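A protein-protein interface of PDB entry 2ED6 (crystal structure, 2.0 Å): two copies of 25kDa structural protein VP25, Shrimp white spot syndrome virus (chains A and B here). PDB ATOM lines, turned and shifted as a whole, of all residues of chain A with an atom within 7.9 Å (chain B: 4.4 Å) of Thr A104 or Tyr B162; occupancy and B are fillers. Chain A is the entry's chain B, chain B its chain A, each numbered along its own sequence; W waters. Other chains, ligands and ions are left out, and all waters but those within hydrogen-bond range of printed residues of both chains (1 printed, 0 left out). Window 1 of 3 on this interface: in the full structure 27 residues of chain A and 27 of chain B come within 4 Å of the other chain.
Water W1 lies within hydrogen-bond range of the side-chain hydroxyl of Tyr B162 (2.6 Å) and the backbone carbonyl oxygen of Phe A127 (2.9 Å).
Positions printed for both chains: 105, 106, 162, 163 and 164.
Tyr B162 touches Thr A104 (CE1 to O, 3.7 Å).
Phe A127 touches Val B109 (CZ to CG2, 3.9 Å).
Phe A127 touches Tyr B162 (CE1 to OH, 3.3 Å).
Pro A129 touches Arg B22 (CD to NH1, 3.6 Å).
Pro A129 touches Tyr B162.
The guanidinium group of Arg B22 is in salt-bridge range of the side-chain carboxylate of Asp B160, at 3.97 Å.
The backbone NH (N) of Tyr B162 sits at hydrogen-bond distance from the backbone carbonyl oxygen (O) of Gln B107.
The backbone carbonyl oxygen of Val B109 sits at hydrogen-bond distance from the backbone NH of Asp B160, 2.9 Å away.
The backbone NH (N) of Thr A104 sits at hydrogen-bond distance from the backbone carbonyl oxygen (O) of His A164 (3.0 Å).
Of the 22 printed residues of chain A, 3 touch a printed residue of chain B.
Hydrophobic or aromatic side chains of chain B that line the printed part of chain A: Val B109 and Tyr B162.
Along chain B the printed residues that touch a printed residue of chain A span positions 22 to 162.
Among the printed residues, no Asp or Glu carboxylate lies within 4 Å of a Lys or Arg side-chain nitrogen of the other chain.
Printed residues of chain B within 4 Å of Phe A127: Val B109 (3.9 Å) and Tyr B162 (3.3 Å).
Printed residues of chain B within 4 Å of Pro A129: Arg B22 and Tyr B162.
Val A165 touches none of the printed residues of chain B.
Of the printed residues of chain A, Arg B22 touches Pro A129 (3.6 Å).
The nearest residue of chain A that does not touch Tyr B162 is Gly A105 (5.9 Å).
The nearest printed residue of chain B that does not touch Pro A129 is Asp B160 (5.4 Å).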
ATOM      1  N   GLU A  19      23.230 -15.118 -20.241  1.00  0.00           N
ATOM      2  CA  GLU A  19      24.235 -14.672 -19.282  1.00  0.00           C
ATOM      3  C   GLU A  19      25.212 -13.618 -19.823  1.00  0.00           C
ATOM      4  O   GLU A  19      25.765 -13.762 -20.918  1.00  0.00           O
ATOM      5  CB  GLU A  19      25.013 -15.882 -18.747  1.00  0.00           C
ATOM      6  CG  GLU A  19      26.082 -15.554 -17.707  1.00  0.00           C
ATOM      7  CD  GLU A  19      25.515 -15.121 -16.365  1.00  0.00           C
ATOM      8  OE1 GLU A  19      26.318 -14.889 -15.436  1.00  0.00           O
ATOM      9  OE2 GLU A  19      24.279 -15.013 -16.233  1.00  0.00           O
ATOM     10  N   ASN A  20      25.393 -12.542 -19.060  1.00  0.00           N
ATOM     11  CA  ASN A  20      26.342 -11.491 -19.421  1.00  0.00           C
ATOM     12  C   ASN A  20      27.534 -11.695 -18.502  1.00  0.00           C
ATOM     13  O   ASN A  20      27.521 -11.255 -17.356  1.00  0.00           O
ATOM     14  CB  ASN A  20      25.763 -10.098 -19.188  1.00  0.00           C
ATOM     15  CG  ASN A  20      24.687  -9.746 -20.182  1.00  0.00           C
ATOM     16  OD1 ASN A  20      24.829  -9.996 -21.379  1.00  0.00           O
ATOM     17  ND2 ASN A  20      23.605  -9.149 -19.698  1.00  0.00           N
ATOM     18  N   ILE A 101      26.684 -23.747 -27.544  1.00  0.00           N
ATOM     19  CA  ILE A 101      26.596 -22.457 -26.875  1.00  0.00           C
ATOM     20  C   ILE A 101      26.936 -21.336 -27.864  1.00  0.00           C
ATOM     21  O   ILE A 101      27.667 -21.550 -28.834  1.00  0.00           O
ATOM     22  CB  ILE A 101      27.535 -22.429 -25.635  1.00  0.00           C
ATOM     23  CG1 ILE A 101      27.079 -21.352 -24.657  1.00  0.00           C
ATOM     24  CG2 ILE A 101      28.982 -22.218 -26.070  1.00  0.00           C
ATOM     25  CD1 ILE A 101      27.732 -21.456 -23.286  1.00  0.00           C
ATOM     26  N   ASN A 102      26.394 -20.144 -27.624  1.00  0.00           N
ATOM     27  CA  ASN A 102      26.622 -19.012 -28.514  1.00  0.00           C
ATOM     28  C   ASN A 102      27.159 -17.771 -27.794  1.00  0.00           C
ATOM     29  O   ASN A 102      26.625 -17.364 -26.763  1.00  0.00           O
ATOM     30  CB  ASN A 102      25.311 -18.648 -29.219  1.00  0.00           C
ATOM     31  CG  ASN A 102      24.638 -19.852 -29.859  1.00  0.00           C
ATOM     32  OD1 ASN A 102      24.988 -20.253 -30.968  1.00  0.00           O
ATOM     33  ND2 ASN A 102      23.678 -20.447 -29.148  1.00  0.00           N
ATOM     34  N   ILE A 103      28.215 -17.181 -28.345  1.00  0.00           N
ATOM     35  CA  ILE A 103      28.819 -15.966 -27.790  1.00  0.00           C
ATOM     36  C   ILE A 103      28.441 -14.920 -28.827  1.00  0.00           C
ATOM     37  O   ILE A 103      28.997 -14.892 -29.928  1.00  0.00           O
ATOM     38  CB  ILE A 103      30.347 -16.102 -27.691  1.00  0.00           C
ATOM     39  CG1 ILE A 103      30.688 -17.403 -26.961  1.00  0.00           C
ATOM     40  CG2 ILE A 103      30.933 -14.916 -26.920  1.00  0.00           C
ATOM     41  CD1 ILE A 103      32.156 -17.697 -26.900  1.00  0.00           C
ATOM     42  N   THR A 104      27.495 -14.054 -28.477  1.00  0.00           N
ATOM     43  CA  THR A 104      26.982 -13.087 -29.437  1.00  0.00           C
ATOM     44  C   THR A 104      27.035 -11.603 -29.133  1.00  0.00           C
ATOM     45  O   THR A 104      26.331 -10.830 -29.790  1.00  0.00           O
ATOM     46  CB  THR A 104      25.524 -13.407 -29.739  1.00  0.00           C
ATOM     47  OG1 THR A 104      24.746 -13.209 -28.548  1.00  0.00           O
ATOM     48  CG2 THR A 104      25.390 -14.856 -30.196  1.00  0.00           C
ATOM     49  N   GLY A 105      27.833 -11.190 -28.153  1.00  0.00           N
ATOM     50  CA  GLY A 105      27.898  -9.771 -27.844  1.00  0.00           C
ATOM     51  C   GLY A 105      29.022  -9.416 -26.898  1.00  0.00           C
ATOM     52  O   GLY A 105      29.507 -10.260 -26.158  1.00  0.00           O
ATOM     53  N   MET A 106      29.447  -8.159 -26.936  1.00  0.00           N
ATOM     54  CA  MET A 106      30.508  -7.698 -26.057  1.00  0.00           C
ATOM     55  C   MET A 106      30.430  -6.193 -25.893  1.00  0.00           C
ATOM     56  O   MET A 106      30.150  -5.464 -26.847  1.00  0.00           O
ATOM     57  CB  MET A 106      31.885  -8.090 -26.607  1.00  0.00           C
ATOM     58  CG  MET A 106      33.082  -7.689 -25.717  1.00  0.00           C
ATOM     59  SD  MET A 106      33.603  -5.930 -25.819  1.00  0.00           S
ATOM     60  CE  MET A 106      34.909  -6.036 -27.007  1.00  0.00           C
ATOM     61  N   PHE A 127      32.892  -7.230 -32.740  1.00  0.00           N
ATOM     62  CA  PHE A 127      33.137  -8.638 -32.463  1.00  0.00           C
ATOM     63  C   PHE A 127      32.505  -9.500 -33.545  1.00  0.00           C
ATOM     64  O   PHE A 127      31.701  -9.022 -34.349  1.00  0.00           O
ATOM     65  CB  PHE A 127      32.540  -9.003 -31.098  1.00  0.00           C
ATOM     66  CG  PHE A 127      31.091  -8.625 -30.953  1.00  0.00           C
ATOM     67  CD1 PHE A 127      30.085  -9.463 -31.425  1.00  0.00           C
ATOM     68  CD2 PHE A 127      30.733  -7.406 -30.385  1.00  0.00           C
ATOM     69  CE1 PHE A 127      28.746  -9.087 -31.336  1.00  0.00           C
ATOM     70  CE2 PHE A 127      29.399  -7.024 -30.293  1.00  0.00           C
ATOM     71  CZ  PHE A 127      28.405  -7.864 -30.770  1.00  0.00           C
ATOM     72  N   THR A 128      32.877 -10.772 -33.560  1.00  0.00           N
ATOM     73  CA  THR A 128      32.333 -11.714 -34.529  1.00  0.00           C
ATOM     74  C   THR A 128      31.699 -12.856 -33.743  1.00  0.00           C
ATOM     75  O   THR A 128      32.405 -13.682 -33.150  1.00  0.00           O
ATOM     76  CB  THR A 128      33.435 -12.277 -35.444  1.00  0.00           C
ATOM     77  OG1 THR A 128      34.083 -11.197 -36.126  1.00  0.00           O
ATOM     78  CG2 THR A 128      32.837 -13.233 -36.478  1.00  0.00           C
ATOM     79  N   PRO A 129      30.359 -12.905 -33.709  1.00  0.00           N
ATOM     80  CA  PRO A 129      29.658 -13.959 -32.976  1.00  0.00           C
ATOM     81  C   PRO A 129      30.162 -15.333 -33.382  1.00  0.00           C
ATOM     82  O   PRO A 129      30.599 -15.530 -34.515  1.00  0.00           O
ATOM     83  CB  PRO A 129      28.198 -13.747 -33.375  1.00  0.00           C
ATOM     84  CG  PRO A 129      28.123 -12.278 -33.613  1.00  0.00           C
ATOM     85  CD  PRO A 129      29.399 -12.006 -34.377  1.00  0.00           C
ATOM     86  N   VAL A 130      30.114 -16.275 -32.452  1.00  0.00           N
ATOM     87  CA  VAL A 130      30.545 -17.630 -32.735  1.00  0.00           C
ATOM     88  C   VAL A 130      29.682 -18.612 -31.953  1.00  0.00           C
ATOM     89  O   VAL A 130      29.282 -18.341 -30.819  1.00  0.00           O
ATOM     90  CB  VAL A 130      32.041 -17.840 -32.357  1.00  0.00           C
ATOM     91  CG1 VAL A 130      32.252 -17.608 -30.859  1.00  0.00           C
ATOM     92  CG2 VAL A 130      32.482 -19.242 -32.737  1.00  0.00           C
ATOM     93  N   SER A 131      29.365 -19.738 -32.582  1.00  0.00           N
ATOM     94  CA  SER A 131      28.581 -20.780 -31.934  1.00  0.00           C
ATOM     95  C   SER A 131      29.547 -21.947 -31.775  1.00  0.00           C
ATOM     96  O   SER A 131      30.274 -22.292 -32.704  1.00  0.00           O
ATOM     97  CB  SER A 131      27.387 -21.178 -32.804  1.00  0.00           C
ATOM     98  OG  SER A 131      27.811 -21.682 -34.056  1.00  0.00           O
ATOM     99  N   PHE A 140      36.208 -16.253 -30.266  1.00  0.00           N
ATOM    100  CA  PHE A 140      35.348 -15.076 -30.302  1.00  0.00           C
ATOM    101  C   PHE A 140      36.254 -13.862 -30.486  1.00  0.00           C
ATOM    102  O   PHE A 140      36.846 -13.373 -29.527  1.00  0.00           O
ATOM    103  CB  PHE A 140      34.578 -14.955 -28.983  1.00  0.00           C
ATOM    104  CG  PHE A 140      33.661 -13.755 -28.910  1.00  0.00           C
ATOM    105  CD1 PHE A 140      32.526 -13.678 -29.706  1.00  0.00           C
ATOM    106  CD2 PHE A 140      33.923 -12.719 -28.018  1.00  0.00           C
ATOM    107  CE1 PHE A 140      31.657 -12.583 -29.614  1.00  0.00           C
ATOM    108  CE2 PHE A 140      33.069 -11.623 -27.916  1.00  0.00           C
ATOM    109  CZ  PHE A 140      31.933 -11.551 -28.713  1.00  0.00           C
ATOM    110  N   TYR A 162      32.071  -7.263 -20.739  1.00  0.00           N
ATOM    111  CA  TYR A 162      30.861  -8.061 -20.581  1.00  0.00           C
ATOM    112  C   TYR A 162      30.622  -8.832 -21.875  1.00  0.00           C
ATOM    113  O   TYR A 162      30.524  -8.239 -22.953  1.00  0.00           O
ATOM    114  CB  TYR A 162      29.669  -7.147 -20.268  1.00  0.00           C
ATOM    115  CG  TYR A 162      29.731  -6.530 -18.885  1.00  0.00           C
ATOM    116  CD1 TYR A 162      29.208  -7.198 -17.774  1.00  0.00           C
ATOM    117  CD2 TYR A 162      30.355  -5.303 -18.680  1.00  0.00           C
ATOM    118  CE1 TYR A 162      29.315  -6.657 -16.489  1.00  0.00           C
ATOM    119  CE2 TYR A 162      30.468  -4.754 -17.403  1.00  0.00           C
ATOM    120  CZ  TYR A 162      29.949  -5.436 -16.314  1.00  0.00           C
ATOM    121  OH  TYR A 162      30.105  -4.910 -15.049  1.00  0.00           O
ATOM    122  N   VAL A 163      30.545 -10.154 -21.776  1.00  0.00           N
ATOM    123  CA  VAL A 163      30.320 -10.983 -22.952  1.00  0.00           C
ATOM    124  C   VAL A 163      28.969 -11.686 -22.841  1.00  0.00           C
ATOM    125  O   VAL A 163      28.672 -12.350 -21.849  1.00  0.00           O
ATOM    126  CB  VAL A 163      31.450 -12.037 -23.135  1.00  0.00           C
ATOM    127  CG1 VAL A 163      32.803 -11.335 -23.216  1.00  0.00           C
ATOM    128  CG2 VAL A 163      31.446 -13.021 -21.989  1.00  0.00           C
ATOM    129  N   HIS A 164      28.142 -11.528 -23.864  1.00  0.00           N
ATOM    130  CA  HIS A 164      26.826 -12.148 -23.839  1.00  0.00           C
ATOM    131  C   HIS A 164      26.887 -13.587 -24.327  1.00  0.00           C
ATOM    132  O   HIS A 164      27.297 -13.859 -25.459  1.00  0.00           O
ATOM    133  CB  HIS A 164      25.835 -11.360 -24.695  1.00  0.00           C
ATOM    134  CG  HIS A 164      24.433 -11.875 -24.603  1.00  0.00           C
ATOM    135  ND1 HIS A 164      23.675 -11.770 -23.456  1.00  0.00           N
ATOM    136  CD2 HIS A 164      23.667 -12.539 -25.501  1.00  0.00           C
ATOM    137  CE1 HIS A 164      22.503 -12.347 -23.652  1.00  0.00           C
ATOM    138  NE2 HIS A 164      22.473 -12.823 -24.885  1.00  0.00           N
ATOM    139  N   VAL A 165      26.470 -14.503 -23.463  1.00  0.00           N
ATOM    140  CA  VAL A 165      26.484 -15.928 -23.778  1.00  0.00           C
ATOM    141  C   VAL A 165      25.059 -16.468 -23.730  1.00  0.00           C
ATOM    142  O   VAL A 165      24.300 -16.179 -22.797  1.00  0.00           O
ATOM    143  CB  VAL A 165      27.353 -16.693 -22.759  1.00  0.00           C
ATOM    144  CG1 VAL A 165      27.440 -18.171 -23.139  1.00  0.00           C
ATOM    145  CG2 VAL A 165      28.747 -16.067 -22.697  1.00  0.00           C
ATOM    146  N   THR A 166      24.683 -17.243 -24.738  1.00  0.00           N
ATOM    147  CA  THR A 166      23.335 -17.790 -24.763  1.00  0.00           C
ATOM    148  C   THR A 166      23.248 -19.173 -25.376  1.00  0.00           C
ATOM    149  O   THR A 166      23.988 -19.497 -26.309  1.00  0.00           O
ATOM    150  CB  THR A 166      22.382 -16.880 -25.551  1.00  0.00           C
ATOM    151  OG1 THR A 166      22.387 -15.570 -24.971  1.00  0.00           O
ATOM    152  CG2 THR A 166      20.976 -17.429 -25.512  1.00  0.00           C
ATOM    153  N   SER A 168      20.398 -20.150 -26.682  1.00  0.00           N
ATOM    154  CA  SER A 168      19.337 -20.062 -27.679  1.00  0.00           C
ATOM    155  C   SER A 168      19.914 -20.529 -29.007  1.00  0.00           C
ATOM    156  O   SER A 168      19.941 -21.721 -29.287  1.00  0.00           O
ATOM    157  CB  SER A 168      18.817 -18.629 -27.804  1.00  0.00           C
ATOM    158  OG  SER A 168      19.836 -17.756 -28.259  1.00  0.00           O
ATOM    159  N   GLY A 169      20.401 -19.608 -29.826  1.00  0.00           N
ATOM    160  CA  GLY A 169      20.966 -20.038 -31.095  1.00  0.00           C
ATOM    161  C   GLY A 169      20.035 -19.829 -32.275  1.00  0.00           C
ATOM    162  O   GLY A 169      18.825 -20.053 -32.181  1.00  0.00           O
ATOM    163  N   THR A 170      20.606 -19.401 -33.395  1.00  0.00           N
ATOM    164  CA  THR A 170      19.833 -19.142 -34.599  1.00  0.00           C
ATOM    165  C   THR A 170      20.478 -19.784 -35.824  1.00  0.00           C
ATOM    166  O   THR A 170      20.939 -19.037 -36.708  1.00  0.00           O
ATOM    167  CB  THR A 170      19.695 -17.628 -34.837  1.00  0.00           C
ATOM    168  OG1 THR A 170      19.148 -17.008 -33.666  1.00  0.00           O
ATOM    169  CG2 THR A 170      18.775 -17.357 -36.012  1.00  0.00           C
ATOM    170  OXT THR A 170      20.517 -21.031 -35.891  1.00  0.00           O
ATOM    171  N   LEU B  21      18.308 -10.424 -31.619  1.00  0.00           N
ATOM    172  CA  LEU B  21      18.278 -10.744 -33.042  1.00  0.00           C
ATOM    173  C   LEU B  21      19.368 -10.007 -33.808  1.00  0.00           C
ATOM    174  O   LEU B  21      19.464  -8.786 -33.720  1.00  0.00           O
ATOM    175  CB  LEU B  21      16.913 -10.366 -33.620  1.00  0.00           C
ATOM    176  CG  LEU B  21      16.039 -11.451 -34.246  1.00  0.00           C
ATOM    177  CD1 LEU B  21      15.918 -12.649 -33.317  1.00  0.00           C
ATOM    178  CD2 LEU B  21      14.668 -10.857 -34.533  1.00  0.00           C
ATOM    179  N   ARG B  22      20.181 -10.744 -34.559  1.00  0.00           N
ATOM    180  CA  ARG B  22      21.240 -10.117 -35.341  1.00  0.00           C
ATOM    181  C   ARG B  22      20.800  -9.935 -36.783  1.00  0.00           C
ATOM    182  O   ARG B  22      20.547 -10.909 -37.491  1.00  0.00           O
ATOM    183  CB  ARG B  22      22.522 -10.943 -35.323  1.00  0.00           C
ATOM    184  CG  ARG B  22      23.674 -10.213 -36.005  1.00  0.00           C
ATOM    185  CD  ARG B  22      24.937 -11.041 -36.094  1.00  0.00           C
ATOM    186  NE  ARG B  22      24.803 -12.133 -37.046  1.00  0.00           N
ATOM    187  CZ  ARG B  22      25.824 -12.845 -37.510  1.00  0.00           C
ATOM    188  NH1 ARG B  22      27.061 -12.576 -37.109  1.00  0.00           N
ATOM    189  NH2 ARG B  22      25.611 -13.826 -38.378  1.00  0.00           N
ATOM    190  N   GLY B 105      15.336  -2.682 -27.502  1.00  0.00           N
ATOM    191  CA  GLY B 105      16.724  -2.268 -27.547  1.00  0.00           C
ATOM    192  C   GLY B 105      17.370  -2.494 -28.895  1.00  0.00           C
ATOM    193  O   GLY B 105      16.917  -3.330 -29.674  1.00  0.00           O
ATOM    194  N   MET B 106      18.430  -1.734 -29.167  1.00  0.00           N
ATOM    195  CA  MET B 106      19.149  -1.855 -30.423  1.00  0.00           C
ATOM    196  C   MET B 106      20.574  -1.344 -30.270  1.00  0.00           C
ATOM    197  O   MET B 106      20.818  -0.350 -29.593  1.00  0.00           O
ATOM    198  CB  MET B 106      18.433  -1.073 -31.532  1.00  0.00           C
ATOM    199  CG  MET B 106      19.075  -1.186 -32.922  1.00  0.00           C
ATOM    200  SD  MET B 106      20.550  -0.116 -33.169  1.00  0.00           S
ATOM    201  CE  MET B 106      19.804   1.283 -33.978  1.00  0.00           C
ATOM    202  N   GLN B 107      21.507  -2.051 -30.892  1.00  0.00           N
ATOM    203  CA  GLN B 107      22.913  -1.678 -30.875  1.00  0.00           C
ATOM    204  C   GLN B 107      23.438  -1.920 -32.284  1.00  0.00           C
ATOM    205  O   GLN B 107      23.119  -2.943 -32.896  1.00  0.00           O
ATOM    206  CB  GLN B 107      23.692  -2.534 -29.876  1.00  0.00           C
ATOM    207  CG  GLN B 107      25.198  -2.354 -29.969  1.00  0.00           C
ATOM    208  CD  GLN B 107      25.955  -3.190 -28.957  1.00  0.00           C
ATOM    209  OE1 GLN B 107      25.724  -4.392 -28.830  1.00  0.00           O
ATOM    210  NE2 GLN B 107      26.872  -2.558 -28.237  1.00  0.00           N
ATOM    211  N   VAL B 109      26.632  -2.614 -34.447  1.00  0.00           N
ATOM    212  CA  VAL B 109      28.016  -3.060 -34.395  1.00  0.00           C
ATOM    213  C   VAL B 109      28.729  -3.035 -35.744  1.00  0.00           C
ATOM    214  O   VAL B 109      28.306  -3.703 -36.685  1.00  0.00           O
ATOM    215  CB  VAL B 109      28.099  -4.495 -33.820  1.00  0.00           C
ATOM    216  CG1 VAL B 109      29.553  -4.887 -33.610  1.00  0.00           C
ATOM    217  CG2 VAL B 109      27.319  -4.587 -32.502  1.00  0.00           C
ATOM    218  N   ASP B 160      26.134  -4.946 -38.123  1.00  0.00           N
ATOM    219  CA  ASP B 160      25.254  -5.999 -37.648  1.00  0.00           C
ATOM    220  C   ASP B 160      24.380  -5.297 -36.624  1.00  0.00           C
ATOM    221  O   ASP B 160      24.872  -4.820 -35.598  1.00  0.00           O
ATOM    222  CB  ASP B 160      26.039  -7.134 -36.986  1.00  0.00           C
ATOM    223  CG  ASP B 160      26.596  -8.112 -37.995  1.00  0.00           C
ATOM    224  OD1 ASP B 160      25.793  -8.688 -38.759  1.00  0.00           O
ATOM    225  OD2 ASP B 160      27.829  -8.305 -38.031  1.00  0.00           O
ATOM    226  N   MET B 161      23.090  -5.189 -36.922  1.00  0.00           N
ATOM    227  CA  MET B 161      22.159  -4.541 -36.007  1.00  0.00           C
ATOM    228  C   MET B 161      21.580  -5.595 -35.078  1.00  0.00           C
ATOM    229  O   MET B 161      20.990  -6.574 -35.535  1.00  0.00           O
ATOM    230  CB  MET B 161      21.030  -3.845 -36.783  1.00  0.00           C
ATOM    231  CG  MET B 161      20.000  -3.131 -35.903  1.00  0.00           C
ATOM    232  SD  MET B 161      18.685  -2.274 -36.847  1.00  0.00           S
ATOM    233  CE  MET B 161      19.279  -0.673 -36.844  1.00  0.00           C
ATOM    234  N   TYR B 162      21.767  -5.400 -33.781  1.00  0.00           N
ATOM    235  CA  TYR B 162      21.245  -6.342 -32.796  1.00  0.00           C
ATOM    236  C   TYR B 162      20.003  -5.726 -32.170  1.00  0.00           C
ATOM    237  O   TYR B 162      20.056  -4.623 -31.628  1.00  0.00           O
ATOM    238  CB  TYR B 162      22.300  -6.626 -31.722  1.00  0.00           C
ATOM    239  CG  TYR B 162      23.464  -7.448 -32.228  1.00  0.00           C
ATOM    240  CD1 TYR B 162      23.417  -8.844 -32.216  1.00  0.00           C
ATOM    241  CD2 TYR B 162      24.589  -6.832 -32.767  1.00  0.00           C
ATOM    242  CE1 TYR B 162      24.468  -9.606 -32.733  1.00  0.00           C
ATOM    243  CE2 TYR B 162      25.646  -7.587 -33.288  1.00  0.00           C
ATOM    244  CZ  TYR B 162      25.575  -8.969 -33.270  1.00  0.00           C
ATOM    245  OH  TYR B 162      26.596  -9.715 -33.815  1.00  0.00           O
ATOM    246  N   VAL B 163      18.876  -6.423 -32.269  1.00  0.00           N
ATOM    247  CA  VAL B 163      17.636  -5.919 -31.692  1.00  0.00           C
ATOM    248  C   VAL B 163      17.185  -6.826 -30.554  1.00  0.00           C
ATOM    249  O   VAL B 163      17.070  -8.036 -30.721  1.00  0.00           O
ATOM    250  CB  VAL B 163      16.509  -5.822 -32.758  1.00  0.00           C
ATOM    251  CG1 VAL B 163      16.964  -4.941 -33.916  1.00  0.00           C
ATOM    252  CG2 VAL B 163      16.143  -7.198 -33.263  1.00  0.00           C
ATOM    253  N   HIS B 164      16.950  -6.238 -29.387  1.00  0.00           N
ATOM    254  CA  HIS B 164      16.528  -7.018 -28.233  1.00  0.00           C
ATOM    255  C   HIS B 164      15.021  -7.231 -28.244  1.00  0.00           C
ATOM    256  O   HIS B 164      14.247  -6.276 -28.234  1.00  0.00           O
ATOM    257  CB  HIS B 164      16.935  -6.329 -26.931  1.00  0.00           C
ATOM    258  CG  HIS B 164      16.637  -7.142 -25.711  1.00  0.00           C
ATOM    259  ND1 HIS B 164      17.317  -8.302 -25.408  1.00  0.00           N
ATOM    260  CD2 HIS B 164      15.709  -6.986 -24.738  1.00  0.00           C
ATOM    261  CE1 HIS B 164      16.821  -8.826 -24.301  1.00  0.00           C
ATOM    262  NE2 HIS B 164      15.845  -8.046 -23.874  1.00  0.00           N
HETATM  263  O   HOH W   1      28.795  -8.704 -34.658  1.00  0.00           O
